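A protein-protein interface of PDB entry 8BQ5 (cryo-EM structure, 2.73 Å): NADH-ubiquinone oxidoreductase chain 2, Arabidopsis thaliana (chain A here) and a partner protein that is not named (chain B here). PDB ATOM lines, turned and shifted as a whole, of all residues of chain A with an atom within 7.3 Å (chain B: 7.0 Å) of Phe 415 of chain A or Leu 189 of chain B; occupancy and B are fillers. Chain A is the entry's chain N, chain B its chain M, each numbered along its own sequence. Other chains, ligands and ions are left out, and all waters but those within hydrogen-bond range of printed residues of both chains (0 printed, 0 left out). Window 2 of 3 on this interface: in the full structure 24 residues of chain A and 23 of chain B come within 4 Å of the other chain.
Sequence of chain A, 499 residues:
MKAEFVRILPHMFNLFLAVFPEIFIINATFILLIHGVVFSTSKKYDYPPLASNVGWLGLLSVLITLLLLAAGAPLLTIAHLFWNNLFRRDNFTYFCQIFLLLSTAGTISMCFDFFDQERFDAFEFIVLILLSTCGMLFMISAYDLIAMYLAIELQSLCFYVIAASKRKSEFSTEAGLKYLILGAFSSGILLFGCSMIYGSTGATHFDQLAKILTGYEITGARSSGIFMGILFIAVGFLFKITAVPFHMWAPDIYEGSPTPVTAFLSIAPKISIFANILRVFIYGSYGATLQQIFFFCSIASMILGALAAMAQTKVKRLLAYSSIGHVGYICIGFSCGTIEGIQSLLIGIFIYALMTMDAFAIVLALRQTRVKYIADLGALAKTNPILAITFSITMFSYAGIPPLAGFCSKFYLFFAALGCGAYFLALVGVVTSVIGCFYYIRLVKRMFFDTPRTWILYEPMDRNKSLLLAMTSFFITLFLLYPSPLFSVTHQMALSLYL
The side-chain sulfur (SG) of Cys 336 of chain A is disulfide-bonded to the side-chain sulfur (SG) of Cys 420 of chain A (2.1 Å).
Lys 410 of chain A touches Leu 182 of chain B (NZ to CD2, 3.8 Å). CD2 of Leu 189 of chain B touches CE1 of Phe 411 of chain A (3.9 Å). Phe 414 of chain A touches Leu 185 of chain B (CD2 to CD2, 3.9 Å). Phe 414 of chain A touches Leu 186 of chain B (CD1 to CD2, 3.5 Å). Leu 189 of chain B touches Phe 414 of chain A. CD1 of Phe 415 of chain A touches CD2 of Leu 189 of chain B, at 3.7 Å. Phe 193 of chain B touches Phe 415 of chain A. Leu 186 of chain B touches Leu 418 of chain A. CD1 of Leu 418 of chain A touches CB of Leu 189 of chain B (3.7 Å). C of Leu 418 of chain A touches CE2 of Phe 193 of chain B, at 3.5 Å.
Phe 415 of chain A touches just these residues of chain B: Leu 189 (3.7 Å) and Phe 193 (3.2 Å). Leu 189 of chain B touches just these residues of chain A: Phe 411 (3.9 Å), Phe 414 (3.6 Å), Phe 415 (3.7 Å) and Leu 418 (3.7 Å). Of the printed residues of chain A, Leu 186 of chain B touches Phe 414 (3.5 Å) and Leu 418 (3.5 Å). Of the printed residues of chain B, Lys 410 of chain A touches Leu 182. Printed residues of chain B within 4 Å of Leu 418 of chain A: Leu 186 (3.5 Å), Leu 189 (3.7 Å) and Phe 193 (3.5 Å). Printed residues of chain A within 4 Å of Leu 182 of chain B: Lys 410 and Phe 414. Cys 420 of chain A touches none of the printed residues of chain B. The nearest residue of chain A that does not touch Leu 189 of chain B is Lys 410 of chain A (6.1 Å).
Printed residues of chain B that touch a printed residue of chain A: Leu 182, Leu 185, Leu 186, Leu 189 and Phe 193. Among the printed residues, 12 pairs touch across the chains. Among the printed residues, no Asp or Glu carboxylate lies within 4 Å of a Lys or Arg side-chain nitrogen of the other chain.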
ATOM      1  N   CYS A 336      37.727 -20.596  14.273  1.00  0.00           N
ATOM      2  CA  CYS A 336      36.483 -19.876  14.539  1.00  0.00           C
ATOM      3  C   CYS A 336      35.805 -20.294  15.839  1.00  0.00           C
ATOM      4  O   CYS A 336      34.992 -19.529  16.365  1.00  0.00           O
ATOM      5  CB  CYS A 336      35.507 -20.033  13.369  1.00  0.00           C
ATOM      6  SG  CYS A 336      35.565 -18.668  12.170  1.00  0.00           S
ATOM      7  N   GLU A 340      29.929 -25.715  14.396  1.00  0.00           N
ATOM      8  CA  GLU A 340      30.036 -25.878  12.953  1.00  0.00           C
ATOM      9  C   GLU A 340      31.482 -25.813  12.486  1.00  0.00           C
ATOM     10  O   GLU A 340      31.833 -26.449  11.489  1.00  0.00           O
ATOM     11  CB  GLU A 340      29.191 -24.822  12.236  1.00  0.00           C
ATOM     12  CG  GLU A 340      27.897 -24.450  12.955  1.00  0.00           C
ATOM     13  CD  GLU A 340      28.078 -23.351  13.985  1.00  0.00           C
ATOM     14  OE1 GLU A 340      27.753 -23.587  15.167  1.00  0.00           O
ATOM     15  OE2 GLU A 340      28.540 -22.253  13.612  1.00  0.00           O
ATOM     16  N   SER A 409      35.116 -27.841   1.312  1.00  0.00           N
ATOM     17  CA  SER A 409      36.146 -27.101   2.031  1.00  0.00           C
ATOM     18  C   SER A 409      36.138 -25.631   1.642  1.00  0.00           C
ATOM     19  O   SER A 409      36.183 -24.752   2.510  1.00  0.00           O
ATOM     20  CB  SER A 409      37.517 -27.719   1.759  1.00  0.00           C
ATOM     21  OG  SER A 409      37.789 -28.768   2.670  1.00  0.00           O
ATOM     22  N   LYS A 410      36.075 -25.347   0.339  1.00  0.00           N
ATOM     23  CA  LYS A 410      35.987 -23.967  -0.126  1.00  0.00           C
ATOM     24  C   LYS A 410      34.750 -23.286   0.440  1.00  0.00           C
ATOM     25  O   LYS A 410      34.806 -22.139   0.919  1.00  0.00           O
ATOM     26  CB  LYS A 410      35.955 -23.945  -1.656  1.00  0.00           C
ATOM     27  CG  LYS A 410      36.033 -22.563  -2.264  1.00  0.00           C
ATOM     28  CD  LYS A 410      36.425 -22.613  -3.729  1.00  0.00           C
ATOM     29  CE  LYS A 410      35.471 -23.488  -4.520  1.00  0.00           C
ATOM     30  NZ  LYS A 410      35.099 -22.872  -5.822  1.00  0.00           N
ATOM     31  N   PHE A 411      33.618 -23.996   0.403  1.00  0.00           N
ATOM     32  CA  PHE A 411      32.366 -23.411   0.855  1.00  0.00           C
ATOM     33  C   PHE A 411      32.448 -23.020   2.318  1.00  0.00           C
ATOM     34  O   PHE A 411      32.053 -21.911   2.691  1.00  0.00           O
ATOM     35  CB  PHE A 411      31.222 -24.395   0.609  1.00  0.00           C
ATOM     36  CG  PHE A 411      29.894 -23.974   1.196  1.00  0.00           C
ATOM     37  CD1 PHE A 411      28.918 -23.420   0.385  1.00  0.00           C
ATOM     38  CD2 PHE A 411      29.594 -24.193   2.533  1.00  0.00           C
ATOM     39  CE1 PHE A 411      27.690 -23.049   0.902  1.00  0.00           C
ATOM     40  CE2 PHE A 411      28.368 -23.821   3.058  1.00  0.00           C
ATOM     41  CZ  PHE A 411      27.416 -23.251   2.240  1.00  0.00           C
ATOM     42  N   TYR A 412      32.965 -23.912   3.171  1.00  0.00           N
ATOM     43  CA  TYR A 412      33.045 -23.563   4.585  1.00  0.00           C
ATOM     44  C   TYR A 412      34.097 -22.493   4.842  1.00  0.00           C
ATOM     45  O   TYR A 412      33.923 -21.659   5.735  1.00  0.00           O
ATOM     46  CB  TYR A 412      33.331 -24.773   5.469  1.00  0.00           C
ATOM     47  CG  TYR A 412      33.626 -24.309   6.877  1.00  0.00           C
ATOM     48  CD1 TYR A 412      32.593 -23.978   7.746  1.00  0.00           C
ATOM     49  CD2 TYR A 412      34.933 -24.154   7.326  1.00  0.00           C
ATOM     50  CE1 TYR A 412      32.852 -23.529   9.024  1.00  0.00           C
ATOM     51  CE2 TYR A 412      35.199 -23.699   8.596  1.00  0.00           C
ATOM     52  CZ  TYR A 412      34.157 -23.393   9.444  1.00  0.00           C
ATOM     53  OH  TYR A 412      34.423 -22.945  10.715  1.00  0.00           O
ATOM     54  N   LEU A 413      35.215 -22.524   4.114  1.00  0.00           N
ATOM     55  CA  LEU A 413      36.214 -21.474   4.281  1.00  0.00           C
ATOM     56  C   LEU A 413      35.569 -20.106   4.118  1.00  0.00           C
ATOM     57  O   LEU A 413      35.669 -19.243   5.001  1.00  0.00           O
ATOM     58  CB  LEU A 413      37.352 -21.672   3.274  1.00  0.00           C
ATOM     59  CG  LEU A 413      38.583 -20.752   3.258  1.00  0.00           C
ATOM     60  CD1 LEU A 413      38.320 -19.399   2.591  1.00  0.00           C
ATOM     61  CD2 LEU A 413      39.123 -20.555   4.661  1.00  0.00           C
ATOM     62  N   PHE A 414      34.833 -19.919   3.021  1.00  0.00           N
ATOM     63  CA  PHE A 414      34.188 -18.627   2.805  1.00  0.00           C
ATOM     64  C   PHE A 414      33.033 -18.386   3.777  1.00  0.00           C
ATOM     65  O   PHE A 414      32.814 -17.245   4.202  1.00  0.00           O
ATOM     66  CB  PHE A 414      33.735 -18.515   1.353  1.00  0.00           C
ATOM     67  CG  PHE A 414      34.876 -18.409   0.388  1.00  0.00           C
ATOM     68  CD1 PHE A 414      35.747 -17.336   0.453  1.00  0.00           C
ATOM     69  CD2 PHE A 414      35.107 -19.396  -0.552  1.00  0.00           C
ATOM     70  CE1 PHE A 414      36.808 -17.231  -0.419  1.00  0.00           C
ATOM     71  CE2 PHE A 414      36.170 -19.298  -1.426  1.00  0.00           C
ATOM     72  CZ  PHE A 414      37.022 -18.214  -1.359  1.00  0.00           C
ATOM     73  N   PHE A 415      32.300 -19.433   4.164  1.00  0.00           N
ATOM     74  CA  PHE A 415      31.137 -19.278   5.082  1.00  0.00           C
ATOM     75  C   PHE A 415      31.600 -18.764   6.449  1.00  0.00           C
ATOM     76  O   PHE A 415      31.044 -17.778   6.934  1.00  0.00           O
ATOM     77  CB  PHE A 415      30.395 -20.606   5.249  1.00  0.00           C
ATOM     78  CG  PHE A 415      29.187 -20.582   6.149  1.00  0.00           C
ATOM     79  CD1 PHE A 415      27.964 -20.133   5.680  1.00  0.00           C
ATOM     80  CD2 PHE A 415      29.265 -21.036   7.456  1.00  0.00           C
ATOM     81  CE1 PHE A 415      26.850 -20.120   6.503  1.00  0.00           C
ATOM     82  CE2 PHE A 415      28.151 -21.024   8.279  1.00  0.00           C
ATOM     83  CZ  PHE A 415      26.948 -20.565   7.801  1.00  0.00           C
ATOM     84  N   ALA A 416      32.591 -19.425   7.046  1.00  0.00           N
ATOM     85  CA  ALA A 416      33.123 -19.023   8.367  1.00  0.00           C
ATOM     86  C   ALA A 416      33.659 -17.592   8.308  1.00  0.00           C
ATOM     87  O   ALA A 416      33.394 -16.842   9.247  1.00  0.00           O
ATOM     88  CB  ALA A 416      34.200 -19.987   8.787  1.00  0.00           C
ATOM     89  N   ALA A 417      34.379 -17.238   7.248  1.00  0.00           N
ATOM     90  CA  ALA A 417      34.959 -15.883   7.117  1.00  0.00           C
ATOM     91  C   ALA A 417      33.848 -14.830   7.110  1.00  0.00           C
ATOM     92  O   ALA A 417      33.945 -13.893   7.899  1.00  0.00           O
ATOM     93  CB  ALA A 417      35.807 -15.790   5.876  1.00  0.00           C
ATOM     94  N   LEU A 418      32.813 -14.999   6.284  1.00  0.00           N
ATOM     95  CA  LEU A 418      31.771 -13.942   6.183  1.00  0.00           C
ATOM     96  C   LEU A 418      30.885 -13.974   7.433  1.00  0.00           C
ATOM     97  O   LEU A 418      30.123 -13.011   7.622  1.00  0.00           O
ATOM     98  CB  LEU A 418      30.974 -14.128   4.888  1.00  0.00           C
ATOM     99  CG  LEU A 418      31.823 -14.190   3.619  1.00  0.00           C
ATOM    100  CD1 LEU A 418      30.952 -14.408   2.396  1.00  0.00           C
ATOM    101  CD2 LEU A 418      32.672 -12.937   3.460  1.00  0.00           C
ATOM    102  N   GLY A 419      30.985 -15.027   8.249  1.00  0.00           N
ATOM    103  CA  GLY A 419      30.241 -15.090   9.520  1.00  0.00           C
ATOM    104  C   GLY A 419      31.090 -14.565  10.662  1.00  0.00           C
ATOM    105  O   GLY A 419      30.657 -13.576  11.286  1.00  0.00           O
ATOM    106  N   CYS A 420      32.273 -15.152  10.889  1.00  0.00           N
ATOM    107  CA  CYS A 420      33.216 -14.689  11.951  1.00  0.00           C
ATOM    108  C   CYS A 420      33.554 -13.212  11.656  1.00  0.00           C
ATOM    109  O   CYS A 420      34.156 -12.581  12.536  1.00  0.00           O
ATOM    110  CB  CYS A 420      34.432 -15.623  12.081  1.00  0.00           C
ATOM    111  SG  CYS A 420      34.089 -17.300  12.716  1.00  0.00           S
ATOM    112  N   GLY A 421      33.181 -12.670  10.480  1.00  0.00           N
ATOM    113  CA  GLY A 421      33.345 -11.234  10.166  1.00  0.00           C
ATOM    114  C   GLY A 421      34.620 -10.918   9.406  1.00  0.00           C
ATOM    115  O   GLY A 421      34.900  -9.725   9.219  1.00  0.00           O
ATOM    116  N   LEU B 139      19.791 -19.393  -5.753  1.00  0.00           N
ATOM    117  CA  LEU B 139      21.096 -18.737  -5.974  1.00  0.00           C
ATOM    118  C   LEU B 139      22.224 -19.763  -5.875  1.00  0.00           C
ATOM    119  O   LEU B 139      23.185 -19.626  -6.646  1.00  0.00           O
ATOM    120  CB  LEU B 139      21.239 -17.695  -4.865  1.00  0.00           C
ATOM    121  CG  LEU B 139      21.004 -16.242  -5.258  1.00  0.00           C
ATOM    122  CD1 LEU B 139      19.531 -15.993  -5.527  1.00  0.00           C
ATOM    123  CD2 LEU B 139      21.486 -15.331  -4.145  1.00  0.00           C
ATOM    124  N   LEU B 140      22.101 -20.770  -5.007  1.00  0.00           N
ATOM    125  CA  LEU B 140      23.191 -21.705  -4.741  1.00  0.00           C
ATOM    126  C   LEU B 140      23.354 -22.715  -5.872  1.00  0.00           C
ATOM    127  O   LEU B 140      24.475 -22.972  -6.327  1.00  0.00           O
ATOM    128  CB  LEU B 140      22.942 -22.415  -3.413  1.00  0.00           C
ATOM    129  CG  LEU B 140      24.060 -23.289  -2.855  1.00  0.00           C
ATOM    130  CD1 LEU B 140      25.399 -22.572  -2.939  1.00  0.00           C
ATOM    131  CD2 LEU B 140      23.733 -23.664  -1.424  1.00  0.00           C
ATOM    132  N   LEU B 182      33.549 -16.983  -7.907  1.00  0.00           N
ATOM    133  CA  LEU B 182      33.874 -16.880  -6.486  1.00  0.00           C
ATOM    134  C   LEU B 182      33.279 -15.617  -5.880  1.00  0.00           C
ATOM    135  O   LEU B 182      32.801 -15.624  -4.736  1.00  0.00           O
ATOM    136  CB  LEU B 182      35.388 -16.896  -6.283  1.00  0.00           C
ATOM    137  CG  LEU B 182      36.136 -18.220  -6.441  1.00  0.00           C
ATOM    138  CD1 LEU B 182      37.630 -17.962  -6.477  1.00  0.00           C
ATOM    139  CD2 LEU B 182      35.786 -19.196  -5.329  1.00  0.00           C
ATOM    140  N   MET B 184      30.541 -14.235  -6.844  1.00  0.00           N
ATOM    141  CA  MET B 184      29.095 -14.550  -6.706  1.00  0.00           C
ATOM    142  C   MET B 184      28.895 -15.386  -5.453  1.00  0.00           C
ATOM    143  O   MET B 184      27.906 -15.161  -4.748  1.00  0.00           O
ATOM    144  CB  MET B 184      28.565 -15.371  -7.884  1.00  0.00           C
ATOM    145  CG  MET B 184      27.112 -15.095  -8.216  1.00  0.00           C
ATOM    146  SD  MET B 184      26.228 -16.535  -8.867  1.00  0.00           S
ATOM    147  CE  MET B 184      27.468 -17.223  -9.962  1.00  0.00           C
ATOM    148  N   LEU B 185      29.794 -16.336  -5.221  1.00  0.00           N
ATOM    149  CA  LEU B 185      29.679 -17.189  -4.040  1.00  0.00           C
ATOM    150  C   LEU B 185      29.725 -16.366  -2.759  1.00  0.00           C
ATOM    151  O   LEU B 185      28.958 -16.614  -1.817  1.00  0.00           O
ATOM    152  CB  LEU B 185      30.798 -18.226  -4.029  1.00  0.00           C
ATOM    153  CG  LEU B 185      30.820 -19.183  -2.837  1.00  0.00           C
ATOM    154  CD1 LEU B 185      29.566 -20.040  -2.802  1.00  0.00           C
ATOM    155  CD2 LEU B 185      32.074 -20.038  -2.873  1.00  0.00           C
ATOM    156  N   LEU B 186      30.643 -15.398  -2.701  1.00  0.00           N
ATOM    157  CA  LEU B 186      30.689 -14.499  -1.552  1.00  0.00           C
ATOM    158  C   LEU B 186      29.356 -13.790  -1.369  1.00  0.00           C
ATOM    159  O   LEU B 186      28.833 -13.704  -0.249  1.00  0.00           O
ATOM    160  CB  LEU B 186      31.810 -13.475  -1.720  1.00  0.00           C
ATOM    161  CG  LEU B 186      33.242 -13.982  -1.856  1.00  0.00           C
ATOM    162  CD1 LEU B 186      34.165 -12.828  -2.195  1.00  0.00           C
ATOM    163  CD2 LEU B 186      33.684 -14.668  -0.579  1.00  0.00           C
ATOM    164  N   ALA B 187      28.733 -13.341  -2.457  1.00  0.00           N
ATOM    165  CA  ALA B 187      27.420 -12.658  -2.362  1.00  0.00           C
ATOM    166  C   ALA B 187      26.356 -13.642  -1.879  1.00  0.00           C
ATOM    167  O   ALA B 187      25.498 -13.228  -1.094  1.00  0.00           O
ATOM    168  CB  ALA B 187      27.028 -12.077  -3.689  1.00  0.00           C
ATOM    169  N   ILE B 188      26.406 -14.891  -2.348  1.00  0.00           N
ATOM    170  CA  ILE B 188      25.363 -15.894  -1.984  1.00  0.00           C
ATOM    171  C   ILE B 188      25.464 -16.177  -0.481  1.00  0.00           C
ATOM    172  O   ILE B 188      24.407 -16.266   0.163  1.00  0.00           O
ATOM    173  CB  ILE B 188      25.492 -17.175  -2.843  1.00  0.00           C
ATOM    174  CG1 ILE B 188      25.035 -16.937  -4.283  1.00  0.00           C
ATOM    175  CG2 ILE B 188      24.771 -18.362  -2.222  1.00  0.00           C
ATOM    176  CD1 ILE B 188      25.729 -17.820  -5.282  1.00  0.00           C
ATOM    177  N   LEU B 189      26.680 -16.262   0.065  1.00  0.00           N
ATOM    178  CA  LEU B 189      26.804 -16.480   1.504  1.00  0.00           C
ATOM    179  C   LEU B 189      26.388 -15.241   2.293  1.00  0.00           C
ATOM    180  O   LEU B 189      25.774 -15.351   3.365  1.00  0.00           O
ATOM    181  CB  LEU B 189      28.230 -16.899   1.855  1.00  0.00           C
ATOM    182  CG  LEU B 189      28.660 -18.214   1.203  1.00  0.00           C
ATOM    183  CD1 LEU B 189      30.150 -18.229   0.916  1.00  0.00           C
ATOM    184  CD2 LEU B 189      28.262 -19.392   2.074  1.00  0.00           C
ATOM    185  N   LEU B 190      26.715 -14.051   1.778  1.00  0.00           N
ATOM    186  CA  LEU B 190      26.240 -12.818   2.397  1.00  0.00           C
ATOM    187  C   LEU B 190      24.722 -12.818   2.524  1.00  0.00           C
ATOM    188  O   LEU B 190      24.171 -12.483   3.579  1.00  0.00           O
ATOM    189  CB  LEU B 190      26.713 -11.615   1.579  1.00  0.00           C
ATOM    190  CG  LEU B 190      28.158 -11.152   1.750  1.00  0.00           C
ATOM    191  CD1 LEU B 190      28.296  -9.710   1.320  1.00  0.00           C
ATOM    192  CD2 LEU B 190      28.542 -11.273   3.206  1.00  0.00           C
ATOM    193  N   ILE B 191      24.021 -13.189   1.451  1.00  0.00           N
ATOM    194  CA  ILE B 191      22.528 -13.253   1.481  1.00  0.00           C
ATOM    195  C   ILE B 191      22.101 -14.321   2.487  1.00  0.00           C
ATOM    196  O   ILE B 191      21.221 -14.030   3.309  1.00  0.00           O
ATOM    197  CB  ILE B 191      21.958 -13.525   0.071  1.00  0.00           C
ATOM    198  CG1 ILE B 191      21.820 -12.229  -0.731  1.00  0.00           C
ATOM    199  CG2 ILE B 191      20.641 -14.285   0.115  1.00  0.00           C
ATOM    200  CD1 ILE B 191      22.265 -12.340  -2.167  1.00  0.00           C
ATOM    201  N   LEU B 192      22.705 -15.503   2.419  1.00  0.00           N
ATOM    202  CA  LEU B 192      22.303 -16.592   3.300  1.00  0.00           C
ATOM    203  C   LEU B 192      22.380 -16.191   4.765  1.00  0.00           C
ATOM    204  O   LEU B 192      21.535 -16.606   5.566  1.00  0.00           O
ATOM    205  CB  LEU B 192      23.177 -17.818   3.035  1.00  0.00           C
ATOM    206  CG  LEU B 192      22.847 -19.162   3.691  1.00  0.00           C
ATOM    207  CD1 LEU B 192      21.526 -19.740   3.205  1.00  0.00           C
ATOM    208  CD2 LEU B 192      23.981 -20.135   3.433  1.00  0.00           C
ATOM    209  N   PHE B 193      23.380 -15.387   5.136  1.00  0.00           N
ATOM    210  CA  PHE B 193      23.518 -15.012   6.541  1.00  0.00           C
ATOM    211  C   PHE B 193      22.336 -14.178   7.018  1.00  0.00           C
ATOM    212  O   PHE B 193      21.874 -14.338   8.154  1.00  0.00           O
ATOM    213  CB  PHE B 193      24.835 -14.275   6.766  1.00  0.00           C
ATOM    214  CG  PHE B 193      25.968 -15.189   7.098  1.00  0.00           C
ATOM    215  CD1 PHE B 193      25.847 -16.103   8.130  1.00  0.00           C
ATOM    216  CD2 PHE B 193      27.143 -15.155   6.370  1.00  0.00           C
ATOM    217  CE1 PHE B 193      26.880 -16.960   8.437  1.00  0.00           C
ATOM    218  CE2 PHE B 193      28.182 -16.009   6.675  1.00  0.00           C
ATOM    219  CZ  PHE B 193      28.048 -16.915   7.708  1.00  0.00           C
ATOM    220  N   GLN B 194      21.841 -13.271   6.177  1.00  0.00           N
ATOM    221  CA  GLN B 194      20.588 -12.590   6.477  1.00  0.00           C
ATOM    222  C   GLN B 194      19.429 -13.574   6.529  1.00  0.00           C
ATOM    223  O   GLN B 194      18.814 -13.777   7.581  1.00  0.00           O
ATOM    224  CB  GLN B 194      20.265 -11.525   5.427  1.00  0.00           C
ATOM    225  CG  GLN B 194      20.889 -10.161   5.617  1.00  0.00           C
ATOM    226  CD  GLN B 194      20.017  -9.079   5.002  1.00  0.00           C
ATOM    227  OE1 GLN B 194      20.425  -7.933   4.869  1.00  0.00           O
ATOM    228  NE2 GLN B 194      18.798  -9.445   4.636  1.00  0.00           N
ATOM    229  N   THR B 198      18.443 -19.478   0.362  1.00  0.00           N
ATOM    230  CA  THR B 198      18.824 -18.925  -0.931  1.00  0.00           C
ATOM    231  C   THR B 198      17.764 -19.180  -1.992  1.00  0.00           C
ATOM    232  O   THR B 198      18.102 -19.355  -3.168  1.00  0.00           O
ATOM    233  CB  THR B 198      20.168 -19.501  -1.384  1.00  0.00           C
ATOM    234  OG1 THR B 198      20.081 -20.929  -1.434  1.00  0.00           O
ATOM    235  CG2 THR B 198      21.272 -19.095  -0.420  1.00  0.00           C
ATOM    236  N   LEU B 216      25.810  -6.029  -1.863  1.00  0.00           N
ATOM    237  CA  LEU B 216      25.409  -7.276  -2.564  1.00  0.00           C
ATOM    238  C   LEU B 216      25.405  -7.032  -4.074  1.00  0.00           C
ATOM    239  O   LEU B 216      25.861  -7.923  -4.807  1.00  0.00           O
ATOM    240  CB  LEU B 216      24.024  -7.698  -2.070  1.00  0.00           C
ATOM    241  CG  LEU B 216      24.006  -8.378  -0.704  1.00  0.00           C
ATOM    242  CD1 LEU B 216      22.585  -8.543  -0.192  1.00  0.00           C
ATOM    243  CD2 LEU B 216      24.722  -9.713  -0.762  1.00  0.00           C
